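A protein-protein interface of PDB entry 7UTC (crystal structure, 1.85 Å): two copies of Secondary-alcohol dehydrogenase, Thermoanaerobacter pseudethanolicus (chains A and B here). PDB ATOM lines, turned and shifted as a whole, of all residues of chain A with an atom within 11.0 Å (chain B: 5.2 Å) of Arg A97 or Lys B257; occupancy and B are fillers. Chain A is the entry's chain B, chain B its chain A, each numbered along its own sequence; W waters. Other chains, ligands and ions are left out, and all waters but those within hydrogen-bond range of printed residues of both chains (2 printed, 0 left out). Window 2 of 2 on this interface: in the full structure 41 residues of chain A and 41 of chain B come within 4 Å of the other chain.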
ATOM      1  N   ASP A  89      26.247 -25.034  -6.693  1.00  0.00           N
ATOM      2  CA  ASP A  89      27.488 -25.270  -7.411  1.00  0.00           C
ATOM      3  C   ASP A  89      28.179 -26.447  -6.729  1.00  0.00           C
ATOM      4  O   ASP A  89      28.446 -26.398  -5.526  1.00  0.00           O
ATOM      5  CB  ASP A  89      28.353 -24.012  -7.400  1.00  0.00           C
ATOM      6  CG  ASP A  89      27.706 -22.845  -8.154  1.00  0.00           C
ATOM      7  OD1 ASP A  89      27.213 -23.069  -9.288  1.00  0.00           O
ATOM      8  OD2 ASP A  89      27.680 -21.709  -7.614  1.00  0.00           O
ATOM      9  N   TRP A  90      28.416 -27.525  -7.467  1.00  0.00           N
ATOM     10  CA  TRP A  90      28.846 -28.761  -6.826  1.00  0.00           C
ATOM     11  C   TRP A  90      30.358 -28.864  -6.637  1.00  0.00           C
ATOM     12  O   TRP A  90      30.813 -29.783  -5.949  1.00  0.00           O
ATOM     13  CB  TRP A  90      28.324 -29.970  -7.610  1.00  0.00           C
ATOM     14  CG  TRP A  90      26.876 -30.230  -7.320  1.00  0.00           C
ATOM     15  CD1 TRP A  90      25.803 -29.782  -8.035  1.00  0.00           C
ATOM     16  CD2 TRP A  90      26.342 -30.965  -6.213  1.00  0.00           C
ATOM     17  NE1 TRP A  90      24.631 -30.206  -7.452  1.00  0.00           N
ATOM     18  CE2 TRP A  90      24.932 -30.934  -6.330  1.00  0.00           C
ATOM     19  CE3 TRP A  90      26.917 -31.653  -5.134  1.00  0.00           C
ATOM     20  CZ2 TRP A  90      24.088 -31.559  -5.412  1.00  0.00           C
ATOM     21  CZ3 TRP A  90      26.076 -32.279  -4.224  1.00  0.00           C
ATOM     22  CH2 TRP A  90      24.674 -32.225  -4.370  1.00  0.00           C
ATOM     23  N   ARG A  91      31.144 -27.946  -7.185  1.00  0.00           N
ATOM     24  CA  ARG A  91      32.596 -27.984  -7.037  1.00  0.00           C
ATOM     25  C   ARG A  91      33.041 -26.892  -6.067  1.00  0.00           C
ATOM     26  O   ARG A  91      33.592 -25.861  -6.459  1.00  0.00           O
ATOM     27  CB  ARG A  91      33.273 -27.847  -8.412  1.00  0.00           C
ATOM     28  CG  ARG A  91      33.104 -29.079  -9.315  1.00  0.00           C
ATOM     29  CD  ARG A  91      33.584 -28.831 -10.752  1.00  0.00           C
ATOM     30  NE  ARG A  91      34.995 -28.465 -10.800  1.00  0.00           N
ATOM     31  CZ  ARG A  91      35.446 -27.219 -10.893  1.00  0.00           C
ATOM     32  NH1 ARG A  91      34.621 -26.192 -11.014  1.00  0.00           N
ATOM     33  NH2 ARG A  91      36.759 -26.999 -10.854  1.00  0.00           N
ATOM     34  N   THR A  92      32.788 -27.125  -4.777  1.00  0.00           N
ATOM     35  CA  THR A  92      33.218 -26.228  -3.708  1.00  0.00           C
ATOM     36  C   THR A  92      33.701 -27.056  -2.526  1.00  0.00           C
ATOM     37  O   THR A  92      33.483 -28.268  -2.459  1.00  0.00           O
ATOM     38  CB  THR A  92      32.097 -25.284  -3.255  1.00  0.00           C
ATOM     39  OG1 THR A  92      31.004 -26.051  -2.740  1.00  0.00           O
ATOM     40  CG2 THR A  92      31.614 -24.408  -4.410  1.00  0.00           C
ATOM     41  N   SER A  93      34.363 -26.387  -1.576  1.00  0.00           N
ATOM     42  CA  SER A  93      34.836 -27.082  -0.380  1.00  0.00           C
ATOM     43  C   SER A  93      33.683 -27.547   0.499  1.00  0.00           C
ATOM     44  O   SER A  93      33.781 -28.607   1.131  1.00  0.00           O
ATOM     45  CB  SER A  93      35.768 -26.182   0.429  1.00  0.00           C
ATOM     46  OG  SER A  93      35.058 -25.070   0.946  1.00  0.00           O
ATOM     47  N   GLU A  94      32.598 -26.767   0.566  1.00  0.00           N
ATOM     48  CA  GLU A  94      31.436 -27.168   1.356  1.00  0.00           C
ATOM     49  C   GLU A  94      30.855 -28.488   0.865  1.00  0.00           C
ATOM     50  O   GLU A  94      30.388 -29.305   1.666  1.00  0.00           O
ATOM     51  CB  GLU A  94      30.359 -26.081   1.322  1.00  0.00           C
ATOM     52  CG  GLU A  94      30.725 -24.794   2.039  1.00  0.00           C
ATOM     53  CD  GLU A  94      31.494 -23.839   1.154  1.00  0.00           C
ATOM     54  OE1 GLU A  94      31.809 -24.211  -0.003  1.00  0.00           O
ATOM     55  OE2 GLU A  94      31.779 -22.709   1.612  1.00  0.00           O
ATOM     56  N   VAL A  95      30.853 -28.708  -0.450  1.00  0.00           N
ATOM     57  CA  VAL A  95      30.390 -29.988  -0.966  1.00  0.00           C
ATOM     58  C   VAL A  95      31.317 -31.107  -0.511  1.00  0.00           C
ATOM     59  O   VAL A  95      30.859 -32.188  -0.121  1.00  0.00           O
ATOM     60  CB  VAL A  95      30.260 -29.933  -2.495  1.00  0.00           C
ATOM     61  CG1 VAL A  95      29.988 -31.320  -3.054  1.00  0.00           C
ATOM     62  CG2 VAL A  95      29.149 -28.965  -2.885  1.00  0.00           C
ATOM     63  N   GLN A  96      32.631 -30.861  -0.521  1.00  0.00           N
ATOM     64  CA  GLN A  96      33.575 -31.858  -0.020  1.00  0.00           C
ATOM     65  C   GLN A  96      33.409 -32.083   1.479  1.00  0.00           C
ATOM     66  O   GLN A  96      33.748 -33.160   1.980  1.00  0.00           O
ATOM     67  CB  GLN A  96      35.020 -31.453  -0.336  1.00  0.00           C
ATOM     68  CG  GLN A  96      35.293 -31.130  -1.796  1.00  0.00           C
ATOM     69  CD  GLN A  96      36.761 -31.295  -2.181  1.00  0.00           C
ATOM     70  OE1 GLN A  96      37.576 -31.781  -1.399  1.00  0.00           O
ATOM     71  NE2 GLN A  96      37.095 -30.900  -3.402  1.00  0.00           N
ATOM     72  N   ARG A  97      32.904 -31.087   2.213  1.00  0.00           N
ATOM     73  CA  ARG A  97      32.574 -31.285   3.620  1.00  0.00           C
ATOM     74  C   ARG A  97      31.240 -31.988   3.824  1.00  0.00           C
ATOM     75  O   ARG A  97      30.912 -32.324   4.963  1.00  0.00           O
ATOM     76  CB  ARG A  97      32.525 -29.950   4.364  1.00  0.00           C
ATOM     77  CG  ARG A  97      33.865 -29.373   4.736  1.00  0.00           C
ATOM     78  CD  ARG A  97      33.748 -28.379   5.883  1.00  0.00           C
ATOM     79  NE  ARG A  97      32.992 -27.185   5.522  1.00  0.00           N
ATOM     80  CZ  ARG A  97      31.783 -26.897   5.987  1.00  0.00           C
ATOM     81  NH1 ARG A  97      31.144 -27.718   6.807  1.00  0.00           N
ATOM     82  NH2 ARG A  97      31.208 -25.751   5.629  1.00  0.00           N
ATOM     83  N   GLY A  98      30.452 -32.177   2.766  1.00  0.00           N
ATOM     84  CA  GLY A  98      29.163 -32.827   2.885  1.00  0.00           C
ATOM     85  C   GLY A  98      27.984 -31.930   3.191  1.00  0.00           C
ATOM     86  O   GLY A  98      27.019 -32.391   3.811  1.00  0.00           O
ATOM     87  N   TYR A  99      28.017 -30.651   2.768  1.00  0.00           N
ATOM     88  CA  TYR A  99      26.904 -29.720   3.000  1.00  0.00           C
ATOM     89  C   TYR A  99      26.671 -28.900   1.730  1.00  0.00           C
ATOM     90  O   TYR A  99      26.966 -27.706   1.657  1.00  0.00           O
ATOM     91  CB  TYR A  99      27.164 -28.818   4.210  1.00  0.00           C
ATOM     92  CG  TYR A  99      27.096 -29.564   5.523  1.00  0.00           C
ATOM     93  CD1 TYR A  99      25.893 -29.686   6.213  1.00  0.00           C
ATOM     94  CD2 TYR A  99      28.232 -30.167   6.061  1.00  0.00           C
ATOM     95  CE1 TYR A  99      25.824 -30.379   7.412  1.00  0.00           C
ATOM     96  CE2 TYR A  99      28.172 -30.860   7.259  1.00  0.00           C
ATOM     97  CZ  TYR A  99      26.966 -30.965   7.931  1.00  0.00           C
ATOM     98  OH  TYR A  99      26.904 -31.657   9.123  1.00  0.00           O
ATOM     99  N   HIS A 100      26.114 -29.558   0.710  1.00  0.00           N
ATOM    100  CA  HIS A 100      25.903 -28.890  -0.567  1.00  0.00           C
ATOM    101  C   HIS A 100      24.954 -27.706  -0.431  1.00  0.00           C
ATOM    102  O   HIS A 100      25.087 -26.723  -1.167  1.00  0.00           O
ATOM    103  CB  HIS A 100      25.380 -29.886  -1.605  1.00  0.00           C
ATOM    104  CG  HIS A 100      23.986 -30.356  -1.341  1.00  0.00           C
ATOM    105  ND1 HIS A 100      23.706 -31.445  -0.542  1.00  0.00           N
ATOM    106  CD2 HIS A 100      22.790 -29.887  -1.772  1.00  0.00           C
ATOM    107  CE1 HIS A 100      22.398 -31.622  -0.491  1.00  0.00           C
ATOM    108  NE2 HIS A 100      21.819 -30.692  -1.228  1.00  0.00           N
ATOM    109  N   GLN A 101      24.010 -27.763   0.517  1.00  0.00           N
ATOM    110  CA  GLN A 101      23.099 -26.641   0.735  1.00  0.00           C
ATOM    111  C   GLN A 101      23.838 -25.340   1.003  1.00  0.00           C
ATOM    112  O   GLN A 101      23.266 -24.260   0.800  1.00  0.00           O
ATOM    113  CB  GLN A 101      22.158 -26.926   1.905  1.00  0.00           C
ATOM    114  CG  GLN A 101      21.280 -28.135   1.726  1.00  0.00           C
ATOM    115  CD  GLN A 101      21.860 -29.370   2.387  1.00  0.00           C
ATOM    116  OE1 GLN A 101      23.006 -29.745   2.142  1.00  0.00           O
ATOM    117  NE2 GLN A 101      21.071 -29.998   3.241  1.00  0.00           N
ATOM    118  N   HIS A 102      25.093 -25.416   1.449  1.00  0.00           N
ATOM    119  CA  HIS A 102      25.866 -24.232   1.802  1.00  0.00           C
ATOM    120  C   HIS A 102      27.064 -24.044   0.888  1.00  0.00           C
ATOM    121  O   HIS A 102      28.037 -23.381   1.263  1.00  0.00           O
ATOM    122  CB  HIS A 102      26.290 -24.307   3.264  1.00  0.00           C
ATOM    123  CG  HIS A 102      25.134 -24.507   4.187  1.00  0.00           C
ATOM    124  ND1 HIS A 102      24.174 -23.539   4.389  1.00  0.00           N
ATOM    125  CD2 HIS A 102      24.754 -25.575   4.927  1.00  0.00           C
ATOM    126  CE1 HIS A 102      23.264 -23.993   5.232  1.00  0.00           C
ATOM    127  NE2 HIS A 102      23.594 -25.226   5.576  1.00  0.00           N
ATOM    128  N   SER A 103      26.994 -24.598  -0.318  1.00  0.00           N
ATOM    129  CA  SER A 103      28.086 -24.526  -1.272  1.00  0.00           C
ATOM    130  C   SER A 103      28.301 -23.090  -1.725  1.00  0.00           C
ATOM    131  O   SER A 103      27.461 -22.526  -2.435  1.00  0.00           O
ATOM    132  CB  SER A 103      27.785 -25.429  -2.461  1.00  0.00           C
ATOM    133  OG  SER A 103      28.848 -25.386  -3.387  1.00  0.00           O
ATOM    134  N   GLY A 104      29.416 -22.492  -1.314  1.00  0.00           N
ATOM    135  CA  GLY A 104      29.703 -21.111  -1.627  1.00  0.00           C
ATOM    136  C   GLY A 104      29.287 -20.117  -0.570  1.00  0.00           C
ATOM    137  O   GLY A 104      29.424 -18.908  -0.791  1.00  0.00           O
ATOM    138  N   GLY A 105      28.786 -20.578   0.567  1.00  0.00           N
ATOM    139  CA  GLY A 105      28.348 -19.671   1.604  1.00  0.00           C
ATOM    140  C   GLY A 105      27.104 -20.176   2.292  1.00  0.00           C
ATOM    141  O   GLY A 105      26.490 -21.142   1.832  1.00  0.00           O
ATOM    142  N   MET A 106      26.727 -19.541   3.400  1.00  0.00           N
ATOM    143  CA  MET A 106      25.532 -19.954   4.121  1.00  0.00           C
ATOM    144  C   MET A 106      24.309 -19.841   3.218  1.00  0.00           C
ATOM    145  O   MET A 106      24.079 -18.802   2.589  1.00  0.00           O
ATOM    146  CB  MET A 106      25.354 -19.104   5.380  1.00  0.00           C
ATOM    147  CG  MET A 106      24.169 -19.520   6.237  1.00  0.00           C
ATOM    148  SD  MET A 106      24.128 -18.688   7.837  1.00  0.00           S
ATOM    149  CE  MET A 106      25.725 -19.143   8.501  1.00  0.00           C
ATOM    150  N   LEU A 107      23.544 -20.930   3.131  1.00  0.00           N
ATOM    151  CA  LEU A 107      22.347 -21.058   2.300  1.00  0.00           C
ATOM    152  C   LEU A 107      22.632 -20.886   0.811  1.00  0.00           C
ATOM    153  O   LEU A 107      21.691 -20.749   0.019  1.00  0.00           O
ATOM    154  CB  LEU A 107      21.253 -20.068   2.732  1.00  0.00           C
ATOM    155  CG  LEU A 107      20.987 -19.914   4.236  1.00  0.00           C
ATOM    156  CD1 LEU A 107      19.867 -18.915   4.475  1.00  0.00           C
ATOM    157  CD2 LEU A 107      20.665 -21.251   4.883  1.00  0.00           C
ATOM    158  N   ALA A 108      23.907 -20.918   0.400  1.00  0.00           N
ATOM    159  CA  ALA A 108      24.261 -20.519  -0.959  1.00  0.00           C
ATOM    160  C   ALA A 108      23.876 -21.558  -2.006  1.00  0.00           C
ATOM    161  O   ALA A 108      23.888 -21.242  -3.202  1.00  0.00           O
ATOM    162  CB  ALA A 108      25.757 -20.220  -1.049  1.00  0.00           C
ATOM    163  N   GLY A 109      23.551 -22.785  -1.592  1.00  0.00           N
ATOM    164  CA  GLY A 109      22.962 -23.739  -2.515  1.00  0.00           C
ATOM    165  C   GLY A 109      21.529 -23.411  -2.882  1.00  0.00           C
ATOM    166  O   GLY A 109      21.016 -23.931  -3.878  1.00  0.00           O
ATOM    167  N   GLY A 292      18.915 -27.514  12.639  1.00  0.00           N
ATOM    168  CA  GLY A 292      18.174 -26.635  11.767  1.00  0.00           C
ATOM    169  C   GLY A 292      18.840 -26.609  10.413  1.00  0.00           C
ATOM    170  O   GLY A 292      20.011 -26.240  10.319  1.00  0.00           O
ATOM    171  N   GLU B 165      36.177 -34.034  13.129  1.00  0.00           N
ATOM    172  CA  GLU B 165      36.854 -34.778  12.083  1.00  0.00           C
ATOM    173  C   GLU B 165      38.355 -34.512  12.142  1.00  0.00           C
ATOM    174  O   GLU B 165      38.812 -33.512  12.702  1.00  0.00           O
ATOM    175  CB  GLU B 165      36.293 -34.399  10.712  1.00  0.00           C
ATOM    176  CG  GLU B 165      34.864 -34.849  10.506  1.00  0.00           C
ATOM    177  CD  GLU B 165      34.227 -34.239   9.275  1.00  0.00           C
ATOM    178  OE1 GLU B 165      34.501 -33.053   8.981  1.00  0.00           O
ATOM    179  OE2 GLU B 165      33.452 -34.954   8.604  1.00  0.00           O
ATOM    180  N   LYS B 234      36.228 -17.827   7.356  1.00  0.00           N
ATOM    181  CA  LYS B 234      35.624 -19.151   7.228  1.00  0.00           C
ATOM    182  C   LYS B 234      34.956 -19.595   8.524  1.00  0.00           C
ATOM    183  O   LYS B 234      33.833 -20.111   8.499  1.00  0.00           O
ATOM    184  CB  LYS B 234      36.674 -20.176   6.798  1.00  0.00           C
ATOM    185  CG  LYS B 234      37.258 -19.922   5.422  1.00  0.00           C
ATOM    186  CD  LYS B 234      38.249 -21.003   5.052  1.00  0.00           C
ATOM    187  CE  LYS B 234      39.361 -21.107   6.086  1.00  0.00           C
ATOM    188  NZ  LYS B 234      40.223 -22.293   5.822  1.00  0.00           N
ATOM    189  N   GLY B 235      35.623 -19.405   9.656  1.00  0.00           N
ATOM    190  CA  GLY B 235      35.122 -19.882  10.928  1.00  0.00           C
ATOM    191  C   GLY B 235      35.776 -21.182  11.360  1.00  0.00           C
ATOM    192  O   GLY B 235      36.729 -21.687  10.755  1.00  0.00           O
ATOM    193  N   VAL B 236      35.237 -21.730  12.443  1.00  0.00           N
ATOM    194  CA  VAL B 236      35.708 -22.991  12.990  1.00  0.00           C
ATOM    195  C   VAL B 236      34.722 -24.091  12.622  1.00  0.00           C
ATOM    196  O   VAL B 236      33.539 -23.850  12.361  1.00  0.00           O
ATOM    197  CB  VAL B 236      35.909 -22.919  14.517  1.00  0.00           C
ATOM    198  CG1 VAL B 236      36.751 -21.714  14.871  1.00  0.00           C
ATOM    199  CG2 VAL B 236      34.571 -22.867  15.222  1.00  0.00           C
ATOM    200  N   ASP B 237      35.237 -25.323  12.594  1.00  0.00           N
ATOM    201  CA  ASP B 237      34.409 -26.492  12.341  1.00  0.00           C
ATOM    202  C   ASP B 237      33.573 -26.868  13.556  1.00  0.00           C
ATOM    203  O   ASP B 237      32.494 -27.453  13.404  1.00  0.00           O
ATOM    204  CB  ASP B 237      35.295 -27.662  11.920  1.00  0.00           C
ATOM    205  CG  ASP B 237      35.996 -27.413  10.599  1.00  0.00           C
ATOM    206  OD1 ASP B 237      35.309 -27.452   9.558  1.00  0.00           O
ATOM    207  OD2 ASP B 237      37.222 -27.157  10.595  1.00  0.00           O
ATOM    208  N   ILE B 255      30.714 -18.014  15.410  1.00  0.00           N
ATOM    209  CA  ILE B 255      32.046 -18.393  14.941  1.00  0.00           C
ATOM    210  C   ILE B 255      32.073 -19.737  14.219  1.00  0.00           C
ATOM    211  O   ILE B 255      33.061 -20.041  13.531  1.00  0.00           O
ATOM    212  CB  ILE B 255      33.057 -18.409  16.107  1.00  0.00           C
ATOM    213  CG1 ILE B 255      32.688 -19.467  17.147  1.00  0.00           C
ATOM    214  CG2 ILE B 255      33.129 -17.044  16.762  1.00  0.00           C
ATOM    215  CD1 ILE B 255      33.642 -19.506  18.321  1.00  0.00           C
ATOM    216  N   VAL B 256      31.027 -20.540  14.332  1.00  0.00           N
ATOM    217  CA  VAL B 256      30.988 -21.858  13.708  1.00  0.00           C
ATOM    218  C   VAL B 256      30.498 -21.724  12.273  1.00  0.00           C
ATOM    219  O   VAL B 256      29.570 -20.960  11.984  1.00  0.00           O
ATOM    220  CB  VAL B 256      30.100 -22.809  14.529  1.00  0.00           C
ATOM    221  CG1 VAL B 256      29.795 -24.065  13.754  1.00  0.00           C
ATOM    222  CG2 VAL B 256      30.788 -23.155  15.818  1.00  0.00           C
ATOM    223  N   LYS B 257      31.136 -22.453  11.364  1.00  0.00           N
ATOM    224  CA  LYS B 257      30.749 -22.419   9.965  1.00  0.00           C
ATOM    225  C   LYS B 257      29.466 -23.222   9.745  1.00  0.00           C
ATOM    226  O   LYS B 257      29.065 -24.021  10.598  1.00  0.00           O
ATOM    227  CB  LYS B 257      31.879 -22.969   9.097  1.00  0.00           C
ATOM    228  CG  LYS B 257      32.149 -24.452   9.284  1.00  0.00           C
ATOM    229  CD  LYS B 257      33.319 -24.915   8.421  1.00  0.00           C
ATOM    230  CE  LYS B 257      34.630 -24.284   8.854  1.00  0.00           C
ATOM    231  NZ  LYS B 257      35.782 -24.990   8.226  1.00  0.00           N
ATOM    232  N   PRO B 258      28.790 -23.013   8.612  1.00  0.00           N
ATOM    233  CA  PRO B 258      27.618 -23.839   8.300  1.00  0.00           C
ATOM    234  C   PRO B 258      27.996 -25.311   8.258  1.00  0.00           C
ATOM    235  O   PRO B 258      29.053 -25.684   7.749  1.00  0.00           O
ATOM    236  CB  PRO B 258      27.180 -23.327   6.925  1.00  0.00           C
ATOM    237  CG  PRO B 258      27.680 -21.919   6.887  1.00  0.00           C
ATOM    238  CD  PRO B 258      28.997 -21.961   7.600  1.00  0.00           C
ATOM    239  N   GLY B 259      27.126 -26.148   8.819  1.00  0.00           N
ATOM    240  CA  GLY B 259      27.419 -27.556   8.960  1.00  0.00           C
ATOM    241  C   GLY B 259      28.260 -27.909  10.162  1.00  0.00           C
ATOM    242  O   GLY B 259      28.405 -29.100  10.470  1.00  0.00           O
ATOM    243  N   GLY B 260      28.822 -26.919  10.852  1.00  0.00           N
ATOM    244  CA  GLY B 260      29.606 -27.169  12.039  1.00  0.00           C
ATOM    245  C   GLY B 260      28.735 -27.454  13.241  1.00  0.00           C
ATOM    246  O   GLY B 260      27.507 -27.475  13.173  1.00  0.00           O
ATOM    247  N   ALA B 286      21.130 -23.164   8.941  1.00  0.00           N
ATOM    248  CA  ALA B 286      22.563 -23.168   8.647  1.00  0.00           C
ATOM    249  C   ALA B 286      23.250 -24.496   8.960  1.00  0.00           C
ATOM    250  O   ALA B 286      24.473 -24.592   8.804  1.00  0.00           O
ATOM    251  CB  ALA B 286      23.262 -22.043   9.415  1.00  0.00           C
ATOM    252  N   LYS B 288      23.929 -25.676  11.771  1.00  0.00           N
ATOM    253  CA  LYS B 288      24.805 -25.507  12.932  1.00  0.00           C
ATOM    254  C   LYS B 288      24.175 -26.237  14.115  1.00  0.00           C
ATOM    255  O   LYS B 288      23.501 -25.658  14.965  1.00  0.00           O
ATOM    256  CB  LYS B 288      25.037 -24.034  13.235  1.00  0.00           C
ATOM    257  CG  LYS B 288      25.666 -23.276  12.085  1.00  0.00           C
ATOM    258  CD  LYS B 288      26.177 -21.923  12.526  1.00  0.00           C
ATOM    259  CE  LYS B 288      26.625 -21.119  11.320  1.00  0.00           C
ATOM    260  NZ  LYS B 288      27.148 -19.793  11.728  1.00  0.00           N
HETATM  261  O   HOH W   1      21.310 -24.050  11.702  1.00  0.00           O
HETATM  262  O   HOH W   2      25.264 -29.953  11.373  1.00  0.00           O
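The backbone carbonyl oxygen of Pro B258 is in hydrogen-bond range of the guanidinium group of Arg A97 (3.0 Å). The backbone carbonyl oxygen (O) of Gly B259 is in hydrogen-bond range of the side-chain hydroxyl (OH) of Tyr A99 (3.3 Å). The backbone carbonyl oxygen of Ala B286 is in hydrogen-bond range of a ring nitrogen (NE2) of His A102 (3.4 Å).
The backbone carbonyl oxygen of Val B236 is in hydrogen-bond range of the backbone NH of Lys B257. NZ of Lys B257 is in salt-bridge range of OD1 of Asp B237, 2.8 Å away. O of Val B256 lies within hydrogen-bond range of NZ of Lys B288 (2.7 Å). O of Ala B286 lies within hydrogen-bond range of N of Gly B259. The backbone NH (N) of Tyr A99 lies within hydrogen-bond range of the backbone carbonyl oxygen (O) of Glu A94 (2.9 Å). N of Leu A107 sits at hydrogen-bond distance from ND1 of His A102 (3.0 Å).
No position is printed for both chains. Of the 9 pairs that touch across the chains among the printed residues, none has its exchanged pair printed and touching as well.
Printed residues of chain B that touch a printed residue of chain A: Lys B257, Pro B258, Gly B259, Ala B286 and Lys B288. Of the 22 printed residues of chain A, 5 touch a printed residue of chain B. Hydrophobic or aromatic side chains of chain A within 4 Å of the printed part of chain B: Tyr A99, His A102 and Met A106. Among the printed residues, no Asp or Glu carboxylate lies within 4 Å of a Lys or Arg side-chain nitrogen of the other chain.
Among the printed residues, merely in contact across the chains: Arg A97 with Lys B257 (3.5 Å), Gly A292 with Ala B286 (3.6 Å), Met A106 with Lys B288 (3.6 Å), His A102 with Pro B258 (3.6 Å), Met A106 with Pro B258 (3.8 Å) and Met A106 with Ala B286 (3.8 Å).
Water W1 lies within hydrogen-bond range of the backbone carbonyl oxygen of Gly A292 (2.9 Å), the backbone NH of Ala B286 (2.9 Å) and the backbone NH of Lys B288 (3.1 Å). Water W2 bridges OH of Tyr A99 (3.3 Å) and O of Gly B259 (3.4 Å).
Arg A97 touches two residues of chain B. Lys B257 touches just one residue of chain A: Arg A97 (3.5 Å). Lys B234 touches none of the printed residues of chain A. No residue of chain A comes within 4 Å of Gly B235. No residue of chain A comes within 4 Å of Val B236. Asp B237 touches none of the printed residues of chain A. No residue of chain A comes within 4 Å of Val B256. Gly B259 touches just one residue of chain A: Tyr A99 (3.3 Å). No residue of chain A comes within 4 Å of Gly B260. Printed residues of chain B within 4 Å of Met A106: Pro B258 (3.8 Å), Ala B286 (3.8 Å) and Lys B288 (3.6 Å). Of the printed residues of chain B, Gly A292 touches Ala B286. Of the printed residues of chain B, Tyr A99 touches Gly B259 (3.3 Å).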
